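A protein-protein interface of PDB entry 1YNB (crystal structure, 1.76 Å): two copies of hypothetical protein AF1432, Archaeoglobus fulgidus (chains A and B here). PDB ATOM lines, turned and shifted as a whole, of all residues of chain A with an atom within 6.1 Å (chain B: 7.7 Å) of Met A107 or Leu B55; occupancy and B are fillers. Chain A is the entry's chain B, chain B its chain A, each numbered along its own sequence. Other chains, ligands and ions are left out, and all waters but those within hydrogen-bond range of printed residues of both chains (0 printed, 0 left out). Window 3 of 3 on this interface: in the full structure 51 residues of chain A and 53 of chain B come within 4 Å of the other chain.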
ATOM      1  N   PHE A  73      -8.073   3.785 -20.894  1.00  0.00           N
ATOM      2  CA  PHE A  73      -9.325   3.671 -21.619  1.00  0.00           C
ATOM      3  C   PHE A  73      -9.327   2.527 -22.615  1.00  0.00           C
ATOM      4  O   PHE A  73     -10.369   2.208 -23.189  1.00  0.00           O
ATOM      5  CB  PHE A  73      -9.620   4.981 -22.371  1.00  0.00           C
ATOM      6  CG  PHE A  73     -10.146   6.077 -21.494  1.00  0.00           C
ATOM      7  CD1 PHE A  73     -11.524   6.236 -21.310  1.00  0.00           C
ATOM      8  CD2 PHE A  73      -9.277   6.890 -20.782  1.00  0.00           C
ATOM      9  CE1 PHE A  73     -12.025   7.198 -20.410  1.00  0.00           C
ATOM     10  CE2 PHE A  73      -9.753   7.858 -19.882  1.00  0.00           C
ATOM     11  CZ  PHE A  73     -11.133   8.010 -19.690  1.00  0.00           C
ATOM     12  N   LEU A 104     -19.282   5.625 -23.892  1.00  0.00           N
ATOM     13  CA  LEU A 104     -18.787   6.993 -23.725  1.00  0.00           C
ATOM     14  C   LEU A 104     -19.746   8.103 -24.143  1.00  0.00           C
ATOM     15  O   LEU A 104     -19.340   9.268 -24.271  1.00  0.00           O
ATOM     16  CB  LEU A 104     -17.463   7.156 -24.470  1.00  0.00           C
ATOM     17  CG  LEU A 104     -16.312   6.324 -23.897  1.00  0.00           C
ATOM     18  CD1 LEU A 104     -15.080   6.484 -24.770  1.00  0.00           C
ATOM     19  CD2 LEU A 104     -16.023   6.768 -22.465  1.00  0.00           C
ATOM     20  N   SER A 105     -21.014   7.762 -24.332  1.00  0.00           N
ATOM     21  CA  SER A 105     -22.018   8.753 -24.734  1.00  0.00           C
ATOM     22  C   SER A 105     -22.023  10.020 -23.865  1.00  0.00           C
ATOM     23  O   SER A 105     -22.272  11.126 -24.359  1.00  0.00           O
ATOM     24  CB  SER A 105     -23.407   8.119 -24.714  1.00  0.00           C
ATOM     25  OG  SER A 105     -23.725   7.620 -23.421  1.00  0.00           O
ATOM     26  N   TRP A 106     -21.739   9.873 -22.578  1.00  0.00           N
ATOM     27  CA  TRP A 106     -21.733  11.029 -21.690  1.00  0.00           C
ATOM     28  C   TRP A 106     -20.711  12.084 -22.112  1.00  0.00           C
ATOM     29  O   TRP A 106     -20.832  13.252 -21.745  1.00  0.00           O
ATOM     30  CB  TRP A 106     -21.441  10.602 -20.250  1.00  0.00           C
ATOM     31  CG  TRP A 106     -20.108   9.973 -20.088  1.00  0.00           C
ATOM     32  CD1 TRP A 106     -19.795   8.660 -20.274  1.00  0.00           C
ATOM     33  CD2 TRP A 106     -18.879  10.644 -19.782  1.00  0.00           C
ATOM     34  NE1 TRP A 106     -18.443   8.470 -20.105  1.00  0.00           N
ATOM     35  CE2 TRP A 106     -17.857   9.671 -19.805  1.00  0.00           C
ATOM     36  CE3 TRP A 106     -18.540  11.979 -19.499  1.00  0.00           C
ATOM     37  CZ2 TRP A 106     -16.513   9.986 -19.554  1.00  0.00           C
ATOM     38  CZ3 TRP A 106     -17.202  12.293 -19.250  1.00  0.00           C
ATOM     39  CH2 TRP A 106     -16.206  11.298 -19.278  1.00  0.00           C
ATOM     40  N   MET A 107     -19.696  11.681 -22.869  1.00  0.00           N
ATOM     41  CA  MET A 107     -18.679  12.631 -23.302  1.00  0.00           C
ATOM     42  C   MET A 107     -19.203  13.483 -24.437  1.00  0.00           C
ATOM     43  O   MET A 107     -19.830  12.975 -25.371  1.00  0.00           O
ATOM     44  CB  MET A 107     -17.414  11.916 -23.773  1.00  0.00           C
ATOM     45  CG  MET A 107     -16.647  11.246 -22.669  1.00  0.00           C
ATOM     46  SD  MET A 107     -15.049  10.641 -23.234  1.00  0.00           S
ATOM     47  CE  MET A 107     -14.024  12.086 -22.925  1.00  0.00           C
ATOM     48  N   GLU A 108     -18.953  14.786 -24.350  1.00  0.00           N
ATOM     49  CA  GLU A 108     -19.393  15.696 -25.395  1.00  0.00           C
ATOM     50  C   GLU A 108     -18.570  15.316 -26.616  1.00  0.00           C
ATOM     51  O   GLU A 108     -19.113  15.024 -27.684  1.00  0.00           O
ATOM     52  CB  GLU A 108     -19.134  17.153 -24.989  1.00  0.00           C
ATOM     53  CG  GLU A 108     -20.040  17.653 -23.860  1.00  0.00           C
ATOM     54  CD  GLU A 108     -19.401  17.557 -22.478  1.00  0.00           C
ATOM     55  OE1 GLU A 108     -18.893  16.471 -22.114  1.00  0.00           O
ATOM     56  OE2 GLU A 108     -19.417  18.578 -21.752  1.00  0.00           O
ATOM     57  N   SER A 109     -17.254  15.300 -26.434  1.00  0.00           N
ATOM     58  CA  SER A 109     -16.326  14.926 -27.494  1.00  0.00           C
ATOM     59  C   SER A 109     -15.251  14.025 -26.883  1.00  0.00           C
ATOM     60  O   SER A 109     -14.668  14.362 -25.848  1.00  0.00           O
ATOM     61  CB  SER A 109     -15.673  16.172 -28.096  1.00  0.00           C
ATOM     62  OG  SER A 109     -14.967  16.900 -27.103  1.00  0.00           O
ATOM     63  N   LYS A 110     -14.998  12.879 -27.507  1.00  0.00           N
ATOM     64  CA  LYS A 110     -13.973  11.978 -26.988  1.00  0.00           C
ATOM     65  C   LYS A 110     -12.612  12.273 -27.614  1.00  0.00           C
ATOM     66  O   LYS A 110     -12.514  12.591 -28.803  1.00  0.00           O
ATOM     67  CB  LYS A 110     -14.372  10.508 -27.197  1.00  0.00           C
ATOM     68  CG  LYS A 110     -15.045  10.183 -28.521  1.00  0.00           C
ATOM     69  CD  LYS A 110     -15.862   8.903 -28.376  1.00  0.00           C
ATOM     70  CE  LYS A 110     -16.675   8.588 -29.620  1.00  0.00           C
ATOM     71  NZ  LYS A 110     -17.599   7.427 -29.417  1.00  0.00           N
ATOM     72  N   PRO A 111     -11.543  12.206 -26.801  1.00  0.00           N
ATOM     73  CA  PRO A 111     -10.173  12.464 -27.254  1.00  0.00           C
ATOM     74  C   PRO A 111      -9.665  11.473 -28.297  1.00  0.00           C
ATOM     75  O   PRO A 111     -10.193  10.363 -28.449  1.00  0.00           O
ATOM     76  CB  PRO A 111      -9.361  12.406 -25.959  1.00  0.00           C
ATOM     77  CG  PRO A 111     -10.342  12.853 -24.931  1.00  0.00           C
ATOM     78  CD  PRO A 111     -11.579  12.088 -25.333  1.00  0.00           C
ATOM     79  N   ILE B  49     -11.353   8.862 -12.800  1.00  0.00           N
ATOM     80  CA  ILE B  49     -12.109   9.959 -12.201  1.00  0.00           C
ATOM     81  C   ILE B  49     -11.353  11.308 -12.291  1.00  0.00           C
ATOM     82  O   ILE B  49     -11.982  12.341 -12.523  1.00  0.00           O
ATOM     83  CB  ILE B  49     -12.399   9.664 -10.720  1.00  0.00           C
ATOM     84  CG1 ILE B  49     -13.424   8.492 -10.674  1.00  0.00           C
ATOM     85  CG2 ILE B  49     -13.011  10.889 -10.023  1.00  0.00           C
ATOM     86  CD1 ILE B  49     -13.673   7.948  -9.187  1.00  0.00           C
ATOM     87  N   ALA B  50     -10.035  11.279 -12.082  1.00  0.00           N
ATOM     88  CA  ALA B  50      -9.236  12.513 -12.103  1.00  0.00           C
ATOM     89  C   ALA B  50      -9.318  13.144 -13.500  1.00  0.00           C
ATOM     90  O   ALA B  50      -9.413  14.371 -13.627  1.00  0.00           O
ATOM     91  CB  ALA B  50      -7.804  12.227 -11.718  1.00  0.00           C
ATOM     92  N   PHE B  51      -9.300  12.297 -14.524  1.00  0.00           N
ATOM     93  CA  PHE B  51      -9.442  12.717 -15.925  1.00  0.00           C
ATOM     94  C   PHE B  51     -10.799  13.428 -16.040  1.00  0.00           C
ATOM     95  O   PHE B  51     -10.898  14.558 -16.535  1.00  0.00           O
ATOM     96  CB  PHE B  51      -9.421  11.487 -16.813  1.00  0.00           C
ATOM     97  CG  PHE B  51      -9.592  11.776 -18.270  1.00  0.00           C
ATOM     98  CD1 PHE B  51      -8.513  12.246 -19.025  1.00  0.00           C
ATOM     99  CD2 PHE B  51     -10.812  11.556 -18.890  1.00  0.00           C
ATOM    100  CE1 PHE B  51      -8.654  12.491 -20.400  1.00  0.00           C
ATOM    101  CE2 PHE B  51     -10.973  11.796 -20.258  1.00  0.00           C
ATOM    102  CZ  PHE B  51      -9.860  12.269 -21.006  1.00  0.00           C
ATOM    103  N   ILE B  52     -11.858  12.775 -15.549  1.00  0.00           N
ATOM    104  CA  ILE B  52     -13.184  13.373 -15.590  1.00  0.00           C
ATOM    105  C   ILE B  52     -13.263  14.712 -14.843  1.00  0.00           C
ATOM    106  O   ILE B  52     -13.877  15.673 -15.343  1.00  0.00           O
ATOM    107  CB  ILE B  52     -14.235  12.414 -14.990  1.00  0.00           C
ATOM    108  CG1 ILE B  52     -14.451  11.226 -15.935  1.00  0.00           C
ATOM    109  CG2 ILE B  52     -15.582  13.137 -14.817  1.00  0.00           C
ATOM    110  CD1 ILE B  52     -15.252  10.065 -15.282  1.00  0.00           C
ATOM    111  N   LEU B  53     -12.686  14.772 -13.648  1.00  0.00           N
ATOM    112  CA  LEU B  53     -12.720  16.011 -12.855  1.00  0.00           C
ATOM    113  C   LEU B  53     -12.070  17.172 -13.606  1.00  0.00           C
ATOM    114  O   LEU B  53     -12.581  18.291 -13.589  1.00  0.00           O
ATOM    115  CB  LEU B  53     -12.008  15.842 -11.513  1.00  0.00           C
ATOM    116  CG  LEU B  53     -12.727  14.931 -10.495  1.00  0.00           C
ATOM    117  CD1 LEU B  53     -11.929  14.829  -9.227  1.00  0.00           C
ATOM    118  CD2 LEU B  53     -14.107  15.465 -10.217  1.00  0.00           C
ATOM    119  N   ALA B  54     -10.942  16.899 -14.251  1.00  0.00           N
ATOM    120  CA  ALA B  54     -10.243  17.947 -14.995  1.00  0.00           C
ATOM    121  C   ALA B  54     -11.098  18.408 -16.155  1.00  0.00           C
ATOM    122  O   ALA B  54     -11.310  19.598 -16.327  1.00  0.00           O
ATOM    123  CB  ALA B  54      -8.891  17.425 -15.493  1.00  0.00           C
ATOM    124  N   LEU B  55     -11.613  17.486 -16.958  1.00  0.00           N
ATOM    125  CA  LEU B  55     -12.421  17.898 -18.084  1.00  0.00           C
ATOM    126  C   LEU B  55     -13.648  18.706 -17.673  1.00  0.00           C
ATOM    127  O   LEU B  55     -13.936  19.777 -18.255  1.00  0.00           O
ATOM    128  CB  LEU B  55     -12.855  16.688 -18.901  1.00  0.00           C
ATOM    129  CG  LEU B  55     -11.782  16.004 -19.754  1.00  0.00           C
ATOM    130  CD1 LEU B  55     -12.455  14.959 -20.640  1.00  0.00           C
ATOM    131  CD2 LEU B  55     -11.049  17.038 -20.631  1.00  0.00           C
ATOM    132  N   LYS B  56     -14.371  18.197 -16.674  1.00  0.00           N
ATOM    133  CA  LYS B  56     -15.571  18.867 -16.185  1.00  0.00           C
ATOM    134  C   LYS B  56     -15.240  20.201 -15.522  1.00  0.00           C
ATOM    135  O   LYS B  56     -16.126  21.019 -15.310  1.00  0.00           O
ATOM    136  CB  LYS B  56     -16.316  17.960 -15.189  1.00  0.00           C
ATOM    137  CG  LYS B  56     -17.032  16.775 -15.839  1.00  0.00           C
ATOM    138  CD  LYS B  56     -18.367  17.193 -16.441  1.00  0.00           C
ATOM    139  CE  LYS B  56     -18.799  16.235 -17.542  1.00  0.00           C
ATOM    140  NZ  LYS B  56     -20.162  16.545 -18.059  1.00  0.00           N
ATOM    141  N   SER B  57     -13.981  20.408 -15.171  1.00  0.00           N
ATOM    142  CA  SER B  57     -13.558  21.658 -14.550  1.00  0.00           C
ATOM    143  C   SER B  57     -13.083  22.625 -15.624  1.00  0.00           C
ATOM    144  O   SER B  57     -12.475  23.646 -15.319  1.00  0.00           O
ATOM    145  CB  SER B  57     -12.414  21.421 -13.570  1.00  0.00           C
ATOM    146  OG  SER B  57     -12.866  20.713 -12.428  1.00  0.00           O
ATOM    147  N   GLY B  58     -13.341  22.270 -16.875  1.00  0.00           N
ATOM    148  CA  GLY B  58     -12.944  23.093 -17.991  1.00  0.00           C
ATOM    149  C   GLY B  58     -11.512  22.952 -18.481  1.00  0.00           C
ATOM    150  O   GLY B  58     -11.169  23.585 -19.489  1.00  0.00           O
ATOM    151  N   GLU B  59     -10.680  22.151 -17.807  1.00  0.00           N
ATOM    152  CA  GLU B  59      -9.279  21.978 -18.218  1.00  0.00           C
ATOM    153  C   GLU B  59      -9.153  21.240 -19.559  1.00  0.00           C
ATOM    154  O   GLU B  59     -10.125  20.657 -20.064  1.00  0.00           O
ATOM    155  CB  GLU B  59      -8.493  21.273 -17.105  1.00  0.00           C
ATOM    156  CG  GLU B  59      -8.612  21.997 -15.753  1.00  0.00           C
ATOM    157  CD  GLU B  59      -7.305  22.616 -15.258  1.00  0.00           C
ATOM    158  OE1 GLU B  59      -6.380  22.829 -16.070  1.00  0.00           O
ATOM    159  OE2 GLU B  59      -7.203  22.906 -14.046  1.00  0.00           O
ATOM    160  N   SER B  60      -7.971  21.304 -20.162  1.00  0.00           N
ATOM    161  CA  SER B  60      -7.746  20.686 -21.472  1.00  0.00           C
ATOM    162  C   SER B  60      -7.546  19.174 -21.391  1.00  0.00           C
ATOM    163  O   SER B  60      -7.224  18.651 -20.335  1.00  0.00           O
ATOM    164  CB  SER B  60      -6.501  21.285 -22.123  1.00  0.00           C
ATOM    165  OG  SER B  60      -5.339  20.861 -21.430  1.00  0.00           O
ATOM    166  N   VAL B  61      -7.729  18.487 -22.510  1.00  0.00           N
ATOM    167  CA  VAL B  61      -7.517  17.048 -22.541  1.00  0.00           C
ATOM    168  C   VAL B  61      -6.104  16.753 -22.056  1.00  0.00           C
ATOM    169  O   VAL B  61      -5.885  15.849 -21.241  1.00  0.00           O
ATOM    170  CB  VAL B  61      -7.688  16.498 -23.953  1.00  0.00           C
ATOM    171  CG1 VAL B  61      -7.367  15.026 -23.979  1.00  0.00           C
ATOM    172  CG2 VAL B  61      -9.100  16.707 -24.400  1.00  0.00           C
ATOM    173  N   GLU B  62      -5.138  17.535 -22.523  1.00  0.00           N
ATOM    174  CA  GLU B  62      -3.761  17.294 -22.124  1.00  0.00           C
ATOM    175  C   GLU B  62      -3.651  17.412 -20.630  1.00  0.00           C
ATOM    176  O   GLU B  62      -2.926  16.657 -19.973  1.00  0.00           O
ATOM    177  CB  GLU B  62      -2.805  18.293 -22.802  1.00  0.00           C
ATOM    178  CG  GLU B  62      -3.070  18.449 -24.297  1.00  0.00           C
ATOM    179  CD  GLU B  62      -4.386  19.162 -24.549  1.00  0.00           C
ATOM    180  OE1 GLU B  62      -5.231  18.672 -25.341  1.00  0.00           O
ATOM    181  OE2 GLU B  62      -4.571  20.232 -23.931  1.00  0.00           O
ATOM    182  N   LYS B  63      -4.382  18.370 -20.086  1.00  0.00           N
ATOM    183  CA  LYS B  63      -4.385  18.613 -18.651  1.00  0.00           C
ATOM    184  C   LYS B  63      -5.098  17.421 -17.951  1.00  0.00           C
ATOM    185  O   LYS B  63      -4.665  16.954 -16.910  1.00  0.00           O
ATOM    186  CB  LYS B  63      -5.150  19.926 -18.380  1.00  0.00           C
ATOM    187  CG  LYS B  63      -4.721  20.706 -17.133  1.00  0.00           C
ATOM    188  CD  LYS B  63      -3.312  21.317 -17.252  1.00  0.00           C
ATOM    189  CE  LYS B  63      -3.123  22.244 -18.486  1.00  0.00           C
ATOM    190  NZ  LYS B  63      -3.976  23.478 -18.522  1.00  0.00           N
ATOM    191  N   ALA B  64      -6.201  16.970 -18.532  1.00  0.00           N
ATOM    192  CA  ALA B  64      -6.968  15.842 -17.975  1.00  0.00           C
ATOM    193  C   ALA B  64      -6.078  14.580 -17.971  1.00  0.00           C
ATOM    194  O   ALA B  64      -6.044  13.840 -16.984  1.00  0.00           O
ATOM    195  CB  ALA B  64      -8.206  15.621 -18.799  1.00  0.00           C
ATOM    196  N   CYS B  65      -5.346  14.342 -19.063  1.00  0.00           N
ATOM    197  CA  CYS B  65      -4.458  13.175 -19.138  1.00  0.00           C
ATOM    198  C   CYS B  65      -3.351  13.259 -18.089  1.00  0.00           C
ATOM    199  O   CYS B  65      -2.873  12.259 -17.562  1.00  0.00           O
ATOM    200  CB  CYS B  65      -3.836  13.077 -20.537  1.00  0.00           C
ATOM    201  SG  CYS B  65      -4.963  12.669 -21.767  1.00  0.00           S
ATOM    202  N   ALA B  67      -3.655  14.654 -15.145  1.00  0.00           N
ATOM    203  CA  ALA B  67      -4.273  14.444 -13.851  1.00  0.00           C
ATOM    204  C   ALA B  67      -4.448  12.929 -13.663  1.00  0.00           C
ATOM    205  O   ALA B  67      -4.247  12.417 -12.567  1.00  0.00           O
ATOM    206  CB  ALA B  67      -5.606  15.158 -13.804  1.00  0.00           C
ATOM    207  N   TYR B 119      -6.873  17.650  -8.353  1.00  0.00           N
ATOM    208  CA  TYR B 119      -7.747  16.682  -9.011  1.00  0.00           C
ATOM    209  C   TYR B 119      -7.424  15.269  -8.506  1.00  0.00           C
ATOM    210  O   TYR B 119      -8.320  14.433  -8.379  1.00  0.00           O
ATOM    211  CB  TYR B 119      -7.594  16.723 -10.536  1.00  0.00           C
ATOM    212  CG  TYR B 119      -8.016  18.043 -11.134  1.00  0.00           C
ATOM    213  CD1 TYR B 119      -9.325  18.515 -10.975  1.00  0.00           C
ATOM    214  CD2 TYR B 119      -7.088  18.861 -11.794  1.00  0.00           C
ATOM    215  CE1 TYR B 119      -9.701  19.770 -11.443  1.00  0.00           C
ATOM    216  CE2 TYR B 119      -7.461  20.125 -12.273  1.00  0.00           C
ATOM    217  CZ  TYR B 119      -8.769  20.572 -12.086  1.00  0.00           C
ATOM    218  OH  TYR B 119      -9.141  21.831 -12.497  1.00  0.00           O
ATOM    219  N   ALA B 155     -16.453  20.313  -9.327  1.00  0.00           N
ATOM    220  CA  ALA B 155     -16.785  19.172 -10.171  1.00  0.00           C
ATOM    221  C   ALA B 155     -16.933  17.910  -9.304  1.00  0.00           C
ATOM    222  O   ALA B 155     -17.845  17.116  -9.505  1.00  0.00           O
ATOM    223  CB  ALA B 155     -15.690  18.952 -11.214  1.00  0.00           C
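The side-chain sulfur (SG) of Cys B65 sits at hydrogen-bond distance from the backbone carbonyl oxygen (O) of Val B61, 3.4 Å away.
CZ of Phe A73 touches CD2 of Phe B51 (3.6 Å).
Trp A106 touches Ile B52 (CH2 to CG1, 3.8 Å).
Met A107 touches Leu B55 (CE to CD1, 3.99 Å).
Phe B51 touches Pro A111.
CG1 of Val B61 touches CG of Pro A111, 3.8 Å away.
Of the printed residues of chain B, Met A107 touches Leu B55 (3.99 Å).
Of the printed residues of chain B, Phe A73 touches Phe B51 (3.6 Å).
Of the printed residues of chain A, Ile B52 touches Trp A106.
Of the printed residues of chain A, Phe B51 touches Phe A73 (3.6 Å) and Pro A111 (3.997 Å).
Of the printed residues of chain B, Trp A106 touches Ile B52.
Ala B67 touches none of the printed residues of chain A.
Tyr B119 touches none of the printed residues of chain A.
The nearest printed residue of chain A that does not touch Leu B55 is Pro A111 (5.2 Å).
The nearest printed residue of chain B that does not touch Pro A111 is Leu B55 (5.2 Å).
Among the printed residues, no Asp or Glu carboxylate lies within 4 Å of a Lys or Arg side-chain nitrogen of the other chain.
No position is printed for both chains.
Of the 5 pairs that touch across the chains among the printed residues, none has its exchanged pair printed and touching as well.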
